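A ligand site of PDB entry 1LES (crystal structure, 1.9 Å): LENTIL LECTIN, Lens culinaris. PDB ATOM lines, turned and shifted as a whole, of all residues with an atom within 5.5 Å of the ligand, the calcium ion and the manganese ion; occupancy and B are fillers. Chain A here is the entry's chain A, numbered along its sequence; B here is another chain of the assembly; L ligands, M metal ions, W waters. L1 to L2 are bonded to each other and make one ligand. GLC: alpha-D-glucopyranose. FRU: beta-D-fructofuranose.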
ATOM      1  N   ALA A  80      28.202   1.054 -12.735  1.00  0.00           N
ATOM      2  CA  ALA A  80      27.066   1.939 -12.497  1.00  0.00           C
ATOM      3  C   ALA A  80      26.321   2.083 -13.848  1.00  0.00           C
ATOM      4  O   ALA A  80      26.798   1.543 -14.832  1.00  0.00           O
ATOM      5  CB  ALA A  80      27.564   3.360 -12.005  1.00  0.00           C
ATOM      6  N   ASP A  81      25.051   2.470 -13.824  1.00  0.00           N
ATOM      7  CA  ASP A  81      24.289   2.789 -12.614  1.00  0.00           C
ATOM      8  C   ASP A  81      23.222   1.759 -12.280  1.00  0.00           C
ATOM      9  O   ASP A  81      22.760   1.687 -11.141  1.00  0.00           O
ATOM     10  CB  ASP A  81      23.631   4.145 -12.763  1.00  0.00           C
ATOM     11  CG  ASP A  81      24.485   5.254 -12.178  1.00  0.00           C
ATOM     12  OD1 ASP A  81      24.498   5.420 -10.921  1.00  0.00           O
ATOM     13  OD2 ASP A  81      25.133   5.942 -12.973  1.00  0.00           O
ATOM     14  N   GLY A  97      19.389  11.062 -15.951  1.00  0.00           N
ATOM     15  CA  GLY A  97      20.268   9.905 -16.074  1.00  0.00           C
ATOM     16  C   GLY A  97      21.103   9.624 -14.822  1.00  0.00           C
ATOM     17  O   GLY A  97      20.737  10.047 -13.718  1.00  0.00           O
ATOM     18  N   GLY A  98      22.215   8.902 -14.969  1.00  0.00           N
ATOM     19  CA  GLY A  98      23.025   8.630 -13.785  1.00  0.00           C
ATOM     20  C   GLY A  98      22.289   7.824 -12.723  1.00  0.00           C
ATOM     21  O   GLY A  98      21.523   6.899 -13.053  1.00  0.00           O
ATOM     22  N   GLY A  99      22.417   8.181 -11.464  1.00  0.00           N
ATOM     23  CA  GLY A  99      21.762   7.383 -10.460  1.00  0.00           C
ATOM     24  C   GLY A  99      20.227   7.501 -10.528  1.00  0.00           C
ATOM     25  O   GLY A  99      19.548   6.806  -9.775  1.00  0.00           O
ATOM     26  N   TYR A 100      19.667   8.393 -11.336  1.00  0.00           N
ATOM     27  CA  TYR A 100      18.204   8.467 -11.393  1.00  0.00           C
ATOM     28  C   TYR A 100      17.608   7.443 -12.350  1.00  0.00           C
ATOM     29  O   TYR A 100      16.397   7.373 -12.552  1.00  0.00           O
ATOM     30  CB  TYR A 100      17.731   9.857 -11.742  1.00  0.00           C
ATOM     31  CG  TYR A 100      17.945  10.804 -10.620  1.00  0.00           C
ATOM     32  CD1 TYR A 100      16.993  10.985  -9.636  1.00  0.00           C
ATOM     33  CD2 TYR A 100      19.122  11.527 -10.553  1.00  0.00           C
ATOM     34  CE1 TYR A 100      17.205  11.879  -8.603  1.00  0.00           C
ATOM     35  CE2 TYR A 100      19.355  12.425  -9.532  1.00  0.00           C
ATOM     36  CZ  TYR A 100      18.400  12.594  -8.576  1.00  0.00           C
ATOM     37  OH  TYR A 100      18.700  13.482  -7.591  1.00  0.00           O
ATOM     38  N   GLU A 119      13.997  -1.585  -9.743  1.00  0.00           N
ATOM     39  CA  GLU A 119      15.411  -1.329 -10.071  1.00  0.00           C
ATOM     40  C   GLU A 119      16.414  -2.402  -9.706  1.00  0.00           C
ATOM     41  O   GLU A 119      16.201  -3.182  -8.789  1.00  0.00           O
ATOM     42  CB  GLU A 119      15.865  -0.010  -9.472  1.00  0.00           C
ATOM     43  CG  GLU A 119      15.698   0.009  -8.004  1.00  0.00           C
ATOM     44  CD  GLU A 119      16.356   1.209  -7.356  1.00  0.00           C
ATOM     45  OE1 GLU A 119      16.048   2.383  -7.674  1.00  0.00           O
ATOM     46  OE2 GLU A 119      17.190   0.946  -6.455  1.00  0.00           O
ATOM     47  N   ASP A 121      19.885  -1.870  -8.999  1.00  0.00           N
ATOM     48  CA  ASP A 121      20.808  -0.754  -8.772  1.00  0.00           C
ATOM     49  C   ASP A 121      22.236  -1.243  -8.441  1.00  0.00           C
ATOM     50  O   ASP A 121      22.471  -1.902  -7.420  1.00  0.00           O
ATOM     51  CB  ASP A 121      20.200   0.067  -7.625  1.00  0.00           C
ATOM     52  CG  ASP A 121      20.883   1.407  -7.399  1.00  0.00           C
ATOM     53  OD1 ASP A 121      22.006   1.632  -7.902  1.00  0.00           O
ATOM     54  OD2 ASP A 121      20.240   2.250  -6.740  1.00  0.00           O
ATOM     55  N   THR A 122      23.212  -0.872  -9.255  1.00  0.00           N
ATOM     56  CA  THR A 122      24.560  -1.344  -9.036  1.00  0.00           C
ATOM     57  C   THR A 122      25.536  -0.319  -8.383  1.00  0.00           C
ATOM     58  O   THR A 122      26.701  -0.646  -8.193  1.00  0.00           O
ATOM     59  CB  THR A 122      25.173  -1.731 -10.356  1.00  0.00           C
ATOM     60  OG1 THR A 122      25.047  -0.623 -11.238  1.00  0.00           O
ATOM     61  CG2 THR A 122      24.515  -3.012 -10.941  1.00  0.00           C
ATOM     62  N   PHE A 123      25.071   0.900  -8.051  1.00  0.00           N
ATOM     63  CA  PHE A 123      25.963   1.946  -7.523  1.00  0.00           C
ATOM     64  C   PHE A 123      25.369   2.683  -6.365  1.00  0.00           C
ATOM     65  O   PHE A 123      24.214   3.129  -6.419  1.00  0.00           O
ATOM     66  CB  PHE A 123      26.308   2.937  -8.629  1.00  0.00           C
ATOM     67  CG  PHE A 123      27.209   4.044  -8.190  1.00  0.00           C
ATOM     68  CD1 PHE A 123      26.669   5.237  -7.637  1.00  0.00           C
ATOM     69  CD2 PHE A 123      28.604   3.911  -8.300  1.00  0.00           C
ATOM     70  CE1 PHE A 123      27.482   6.285  -7.189  1.00  0.00           C
ATOM     71  CE2 PHE A 123      29.430   4.948  -7.867  1.00  0.00           C
ATOM     72  CZ  PHE A 123      28.849   6.143  -7.311  1.00  0.00           C
ATOM     73  N   TYR A 124      26.170   2.835  -5.300  1.00  0.00           N
ATOM     74  CA  TYR A 124      25.654   3.476  -4.096  1.00  0.00           C
ATOM     75  C   TYR A 124      25.596   4.951  -4.159  1.00  0.00           C
ATOM     76  O   TYR A 124      26.646   5.591  -4.246  1.00  0.00           O
ATOM     77  CB  TYR A 124      26.478   3.045  -2.874  1.00  0.00           C
ATOM     78  CG  TYR A 124      26.184   3.851  -1.607  1.00  0.00           C
ATOM     79  CD1 TYR A 124      24.980   3.726  -0.944  1.00  0.00           C
ATOM     80  CD2 TYR A 124      27.141   4.716  -1.070  1.00  0.00           C
ATOM     81  CE1 TYR A 124      24.729   4.453   0.229  1.00  0.00           C
ATOM     82  CE2 TYR A 124      26.890   5.440   0.085  1.00  0.00           C
ATOM     83  CZ  TYR A 124      25.695   5.296   0.723  1.00  0.00           C
ATOM     84  OH  TYR A 124      25.397   6.028   1.840  1.00  0.00           O
ATOM     85  N   ASN A 125      24.392   5.535  -4.218  1.00  0.00           N
ATOM     86  CA  ASN A 125      24.201   7.009  -4.238  1.00  0.00           C
ATOM     87  C   ASN A 125      23.860   7.368  -2.790  1.00  0.00           C
ATOM     88  O   ASN A 125      22.757   7.120  -2.293  1.00  0.00           O
ATOM     89  CB  ASN A 125      23.068   7.481  -5.191  1.00  0.00           C
ATOM     90  CG  ASN A 125      23.323   7.103  -6.638  1.00  0.00           C
ATOM     91  OD1 ASN A 125      22.950   5.996  -7.094  1.00  0.00           O
ATOM     92  ND2 ASN A 125      24.059   7.968  -7.358  1.00  0.00           N
ATOM     93  N   TRP A 128      20.467   8.722  -1.168  1.00  0.00           N
ATOM     94  CA  TRP A 128      19.194   7.983  -1.005  1.00  0.00           C
ATOM     95  C   TRP A 128      19.292   6.475  -0.958  1.00  0.00           C
ATOM     96  O   TRP A 128      18.334   5.810  -0.539  1.00  0.00           O
ATOM     97  CB  TRP A 128      18.151   8.340  -2.126  1.00  0.00           C
ATOM     98  CG  TRP A 128      18.663   8.050  -3.593  1.00  0.00           C
ATOM     99  CD1 TRP A 128      18.803   6.804  -4.191  1.00  0.00           C
ATOM    100  CD2 TRP A 128      19.177   9.000  -4.549  1.00  0.00           C
ATOM    101  NE1 TRP A 128      19.406   6.946  -5.427  1.00  0.00           N
ATOM    102  CE2 TRP A 128      19.630   8.274  -5.674  1.00  0.00           C
ATOM    103  CE3 TRP A 128      19.303  10.406  -4.562  1.00  0.00           C
ATOM    104  CZ2 TRP A 128      20.192   8.888  -6.792  1.00  0.00           C
ATOM    105  CZ3 TRP A 128      19.861  11.010  -5.691  1.00  0.00           C
ATOM    106  CH2 TRP A 128      20.291  10.242  -6.778  1.00  0.00           C
ATOM    107  N   ASP A 129      20.381   5.903  -1.447  1.00  0.00           N
ATOM    108  CA  ASP A 129      20.463   4.450  -1.453  1.00  0.00           C
ATOM    109  C   ASP A 129      20.630   3.842  -0.067  1.00  0.00           C
ATOM    110  O   ASP A 129      21.091   4.511   0.854  1.00  0.00           O
ATOM    111  CB  ASP A 129      21.571   4.041  -2.392  1.00  0.00           C
ATOM    112  CG  ASP A 129      21.107   3.991  -3.836  1.00  0.00           C
ATOM    113  OD1 ASP A 129      19.886   3.777  -4.003  1.00  0.00           O
ATOM    114  OD2 ASP A 129      21.914   4.120  -4.773  1.00  0.00           O
ATOM    115  N   PRO A 130      20.238   2.581   0.125  1.00  0.00           N
ATOM    116  CA  PRO A 130      20.375   1.964   1.452  1.00  0.00           C
ATOM    117  C   PRO A 130      21.808   2.027   2.028  1.00  0.00           C
ATOM    118  O   PRO A 130      22.785   1.700   1.334  1.00  0.00           O
ATOM    119  CB  PRO A 130      19.845   0.534   1.237  1.00  0.00           C
ATOM    120  CG  PRO A 130      20.003   0.305  -0.237  1.00  0.00           C
ATOM    121  CD  PRO A 130      19.691   1.630  -0.857  1.00  0.00           C
ATOM    122  N   HIS A 136      21.555  -3.592  -4.937  1.00  0.00           N
ATOM    123  CA  HIS A 136      20.265  -4.035  -4.479  1.00  0.00           C
ATOM    124  C   HIS A 136      19.171  -3.981  -5.537  1.00  0.00           C
ATOM    125  O   HIS A 136      19.239  -3.204  -6.494  1.00  0.00           O
ATOM    126  CB  HIS A 136      19.813  -3.084  -3.341  1.00  0.00           C
ATOM    127  CG  HIS A 136      19.870  -1.621  -3.703  1.00  0.00           C
ATOM    128  ND1 HIS A 136      21.054  -0.892  -3.714  1.00  0.00           N
ATOM    129  CD2 HIS A 136      18.902  -0.751  -4.068  1.00  0.00           C
ATOM    130  CE1 HIS A 136      20.794   0.355  -4.057  1.00  0.00           C
ATOM    131  NE2 HIS A 136      19.490   0.470  -4.281  1.00  0.00           N
ATOM    132  N   ILE A 144      13.109   7.997  -6.678  1.00  0.00           N
ATOM    133  CA  ILE A 144      14.307   7.112  -6.831  1.00  0.00           C
ATOM    134  C   ILE A 144      14.674   6.439  -5.484  1.00  0.00           C
ATOM    135  O   ILE A 144      15.460   5.482  -5.414  1.00  0.00           O
ATOM    136  CB  ILE A 144      15.521   7.892  -7.422  1.00  0.00           C
ATOM    137  CG1 ILE A 144      16.630   6.928  -7.846  1.00  0.00           C
ATOM    138  CG2 ILE A 144      16.000   8.945  -6.416  1.00  0.00           C
ATOM    139  CD1 ILE A 144      16.214   5.939  -8.962  1.00  0.00           C
ATOM    140  N   SER A 146      13.761   3.902  -3.094  1.00  0.00           N
ATOM    141  CA  SER A 146      12.856   2.750  -2.989  1.00  0.00           C
ATOM    142  C   SER A 146      12.008   2.617  -1.746  1.00  0.00           C
ATOM    143  O   SER A 146      12.418   3.009  -0.666  1.00  0.00           O
ATOM    144  CB  SER A 146      13.655   1.471  -3.121  1.00  0.00           C
ATOM    145  OG  SER A 146      14.581   1.617  -4.169  1.00  0.00           O
ATOM    146  N   THR B  28      24.255   5.074 -17.127  1.00  0.00           N
ATOM    147  CA  THR B  28      25.626   5.050 -16.606  1.00  0.00           C
ATOM    148  C   THR B  28      25.889   6.524 -16.209  1.00  0.00           C
ATOM    149  O   THR B  28      25.086   7.411 -16.495  1.00  0.00           O
ATOM    150  CB  THR B  28      26.649   4.639 -17.648  1.00  0.00           C
ATOM    151  OG1 THR B  28      26.656   5.611 -18.686  1.00  0.00           O
ATOM    152  CG2 THR B  28      26.374   3.227 -18.205  1.00  0.00           C
ATOM    153  N   GLY B  29      27.026   6.804 -15.575  1.00  0.00           N
ATOM    154  CA  GLY B  29      27.302   8.180 -15.163  1.00  0.00           C
ATOM    155  C   GLY B  29      28.804   8.296 -15.155  1.00  0.00           C
ATOM    156  O   GLY B  29      29.407   8.072 -16.201  1.00  0.00           O
ATOM    157  N   ALA B  30      29.417   8.677 -14.023  1.00  0.00           N
ATOM    158  CA  ALA B  30      30.895   8.757 -13.943  1.00  0.00           C
ATOM    159  C   ALA B  30      31.428   7.340 -13.987  1.00  0.00           C
ATOM    160  O   ALA B  30      32.564   7.111 -14.406  1.00  0.00           O
ATOM    161  CB  ALA B  30      31.330   9.476 -12.661  1.00  0.00           C
ATOM    162  N   GLU B  31      30.657   6.359 -13.534  1.00  0.00           N
ATOM    163  CA  GLU B  31      31.068   4.960 -13.685  1.00  0.00           C
ATOM    164  C   GLU B  31      30.138   4.299 -14.720  1.00  0.00           C
ATOM    165  O   GLU B  31      29.119   4.902 -15.094  1.00  0.00           O
ATOM    166  CB  GLU B  31      31.067   4.210 -12.355  1.00  0.00           C
ATOM    167  CG  GLU B  31      32.391   4.407 -11.638  1.00  0.00           C
ATOM    168  CD  GLU B  31      32.277   4.063 -10.203  1.00  0.00           C
ATOM    169  OE1 GLU B  31      31.842   2.911  -9.904  1.00  0.00           O
ATOM    170  OE2 GLU B  31      32.597   4.970  -9.380  1.00  0.00           O
ATOM    171  N   PHE B  32      30.408   3.050 -15.089  1.00  0.00           N
ATOM    172  CA  PHE B  32      29.637   2.494 -16.150  1.00  0.00           C
ATOM    173  C   PHE B  32      29.665   1.010 -16.364  1.00  0.00           C
ATOM    174  O   PHE B  32      30.405   0.263 -15.666  1.00  0.00           O
ATOM    175  CB  PHE B  32      30.025   3.214 -17.455  1.00  0.00           C
ATOM    176  CG  PHE B  32      31.513   3.133 -17.796  1.00  0.00           C
ATOM    177  CD1 PHE B  32      32.040   1.987 -18.405  1.00  0.00           C
ATOM    178  CD2 PHE B  32      32.394   4.164 -17.419  1.00  0.00           C
ATOM    179  CE1 PHE B  32      33.382   1.864 -18.614  1.00  0.00           C
ATOM    180  CE2 PHE B  32      33.724   4.049 -17.630  1.00  0.00           C
ATOM    181  CZ  PHE B  32      34.226   2.893 -18.220  1.00  0.00           C
HETATM  182  C1  GLC L   1      28.094  10.543 -10.971  1.00  0.00           C
HETATM  183  C2  GLC L   1      26.604  10.807 -11.354  1.00  0.00           C
HETATM  184  C3  GLC L   1      25.700   9.968 -10.564  1.00  0.00           C
HETATM  185  C4  GLC L   1      26.007   8.553 -10.857  1.00  0.00           C
HETATM  186  C5  GLC L   1      27.512   8.177 -10.527  1.00  0.00           C
HETATM  187  C6  GLC L   1      27.842   6.721 -10.912  1.00  0.00           C
HETATM  188  O2  GLC L   1      26.316  12.140 -11.074  1.00  0.00           O
HETATM  189  O3  GLC L   1      24.274  10.222 -10.913  1.00  0.00           O
HETATM  190  O4  GLC L   1      25.130   7.805 -10.001  1.00  0.00           O
HETATM  191  O5  GLC L   1      28.283   9.167 -11.265  1.00  0.00           O
HETATM  192  O6  GLC L   1      27.896   6.613 -12.267  1.00  0.00           O
HETATM  193  C1  FRU L   2      29.396  13.003  -9.516  1.00  0.00           C
HETATM  194  C2  FRU L   2      29.364  11.548  -9.073  1.00  0.00           C
HETATM  195  C3  FRU L   2      29.433  11.546  -7.598  1.00  0.00           C
HETATM  196  C4  FRU L   2      29.855  10.092  -7.438  1.00  0.00           C
HETATM  197  C5  FRU L   2      30.965   9.938  -8.367  1.00  0.00           C
HETATM  198  C6  FRU L   2      31.010   8.488  -8.658  1.00  0.00           C
HETATM  199  O1  FRU L   2      30.688  13.595  -9.250  1.00  0.00           O
HETATM  200  O2  FRU L   2      28.179  10.760  -9.550  1.00  0.00           O
HETATM  201  O3  FRU L   2      28.172  11.611  -7.003  1.00  0.00           O
HETATM  202  O4  FRU L   2      30.369   9.836  -6.114  1.00  0.00           O
HETATM  203  O5  FRU L   2      30.562  10.804  -9.430  1.00  0.00           O
HETATM  204  O6  FRU L   2      32.161   8.290  -9.436  1.00  0.00           O
HETATM  205 CA    CA M   1      22.104   3.906  -7.091  1.00  0.00          CA
HETATM  206 MN    MN M   2      18.701   2.291  -5.209  1.00  0.00          MN
HETATM  207  O   HOH W   1      22.961  11.692  -8.931  1.00  0.00           O
HETATM  208  O   HOH W   2      24.629  12.559 -13.650  1.00  0.00           O
HETATM  209  O   HOH W   3      31.481   7.025  -4.997  1.00  0.00           O
HETATM  210  O   HOH W   4      26.289   9.932  -5.925  1.00  0.00           O
HETATM  211  O   HOH W   5      22.315  12.242 -12.389  1.00  0.00           O
HETATM  212  O   HOH W   6      26.219  13.108  -8.459  1.00  0.00           O
HETATM  213  O   HOH W   7      17.695   3.983  -6.315  1.00  0.00           O
HETATM  214  O   HOH W   8      28.426  13.366  -4.872  1.00  0.00           O
HETATM  215  O   HOH W   9      22.648   3.903  -9.261  1.00  0.00           O
HETATM  216  O   HOH W  10      17.339   2.411  -3.758  1.00  0.00           O
HETATM  217  O   HOH W  11      20.019   5.039  -7.667  1.00  0.00           O
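Of the 23 residues printed, 4 come within 4 Å of the manganese ion. The nearest printed residue that does not touch the manganese ion is Ser 146 (4.3 Å).
The manganese ion is bound by water W10, at 2.0 Å. OD2 of Asp 121 is bound to the manganese ion, 2.2 Å away. NE2 of His 136 binds the manganese ion (2.2 Å). The side-chain carboxylate (OD1) of Asp 129 binds the manganese ion, 2.3 Å away. Water W7 binds the manganese ion. OE2 of Glu 119 binds the manganese ion (2.4 Å).
The side-chain amide nitrogen (ND2) of Asn 125 sits at hydrogen-bond distance from an oxygen (O4) of GLC L1, 2.9 Å away. O4 of GLC L1 sits at hydrogen-bond distance from OD1 of Asp 81 (2.6 Å). O3 of GLC L1 is in hydrogen-bond range of N of Gly 99 (2.8 Å). The backbone NH (N) of Ala 30 of chain B is in hydrogen-bond range of an oxygen (O5) of GLC L1. N of Glu 31 of chain B lies within hydrogen-bond range of O6 of GLC L1, at 3.0 Å. The side-chain carboxylate (OE2) of Glu 31 of chain B lies within hydrogen-bond range of an oxygen (O6) of FRU L2 (3.3 Å). N of Gly 29 of chain B sits close to O6 of GLC L1, 3.4 Å away.
CB of Ala 80 touches O6 of GLC L1, 3.3 Å away. CA of Gly 98 touches O3 of GLC L1, at 3.5 Å. Hydrophobic or aromatic side chains that line the ligand: Ala 80, Phe 123 and Ala 30 of chain B. Within 4 Å of the ligand: Ala 80, Asp 81, Gly 98, Gly 99, Phe 123, Asn 125, Gly 29 of chain B, Ala 30 of chain B and Glu 31 of chain B.
The calcium ion is bound by water W9 (2.2 Å), OD1 of Asn 125 (2.3 Å), OD2 of Asp 129 (2.3 Å), O of Phe 123 (2.3 Å), OD1 of Asp 121 (2.4 Å), water W11 (2.4 Å) and OD2 of Asp 121 (2.5 Å).
Water W11 bridges the backbone carbonyl oxygen (O) of Gly 99 and the indole nitrogen (NE1) of Trp 128. Water W7 lies within hydrogen-bond range of the side-chain carboxylate (OE1) of Glu 119 (2.7 Å) and the backbone carbonyl oxygen (O) of Ile 144 (2.8 Å). Water W4 lies within hydrogen-bond range of an oxygen (O3) of FRU L2 (2.7 Å) and the side-chain amide nitrogen (ND2) of Asn 125 (3.3 Å). Water W5 bridges the backbone carbonyl oxygen (O) of Gly 97 and an oxygen (O3) of GLC L1.
N of Gly 99 sits close to OD1 of Asp 81, 3.5 Å away. The side-chain carboxylate of Asp 81 is in hydrogen-bond range of the backbone NH of Gly 29 of chain B, 3.3 Å away. O of Asp 81 is in hydrogen-bond range of N of Thr 122, 3.2 Å away.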
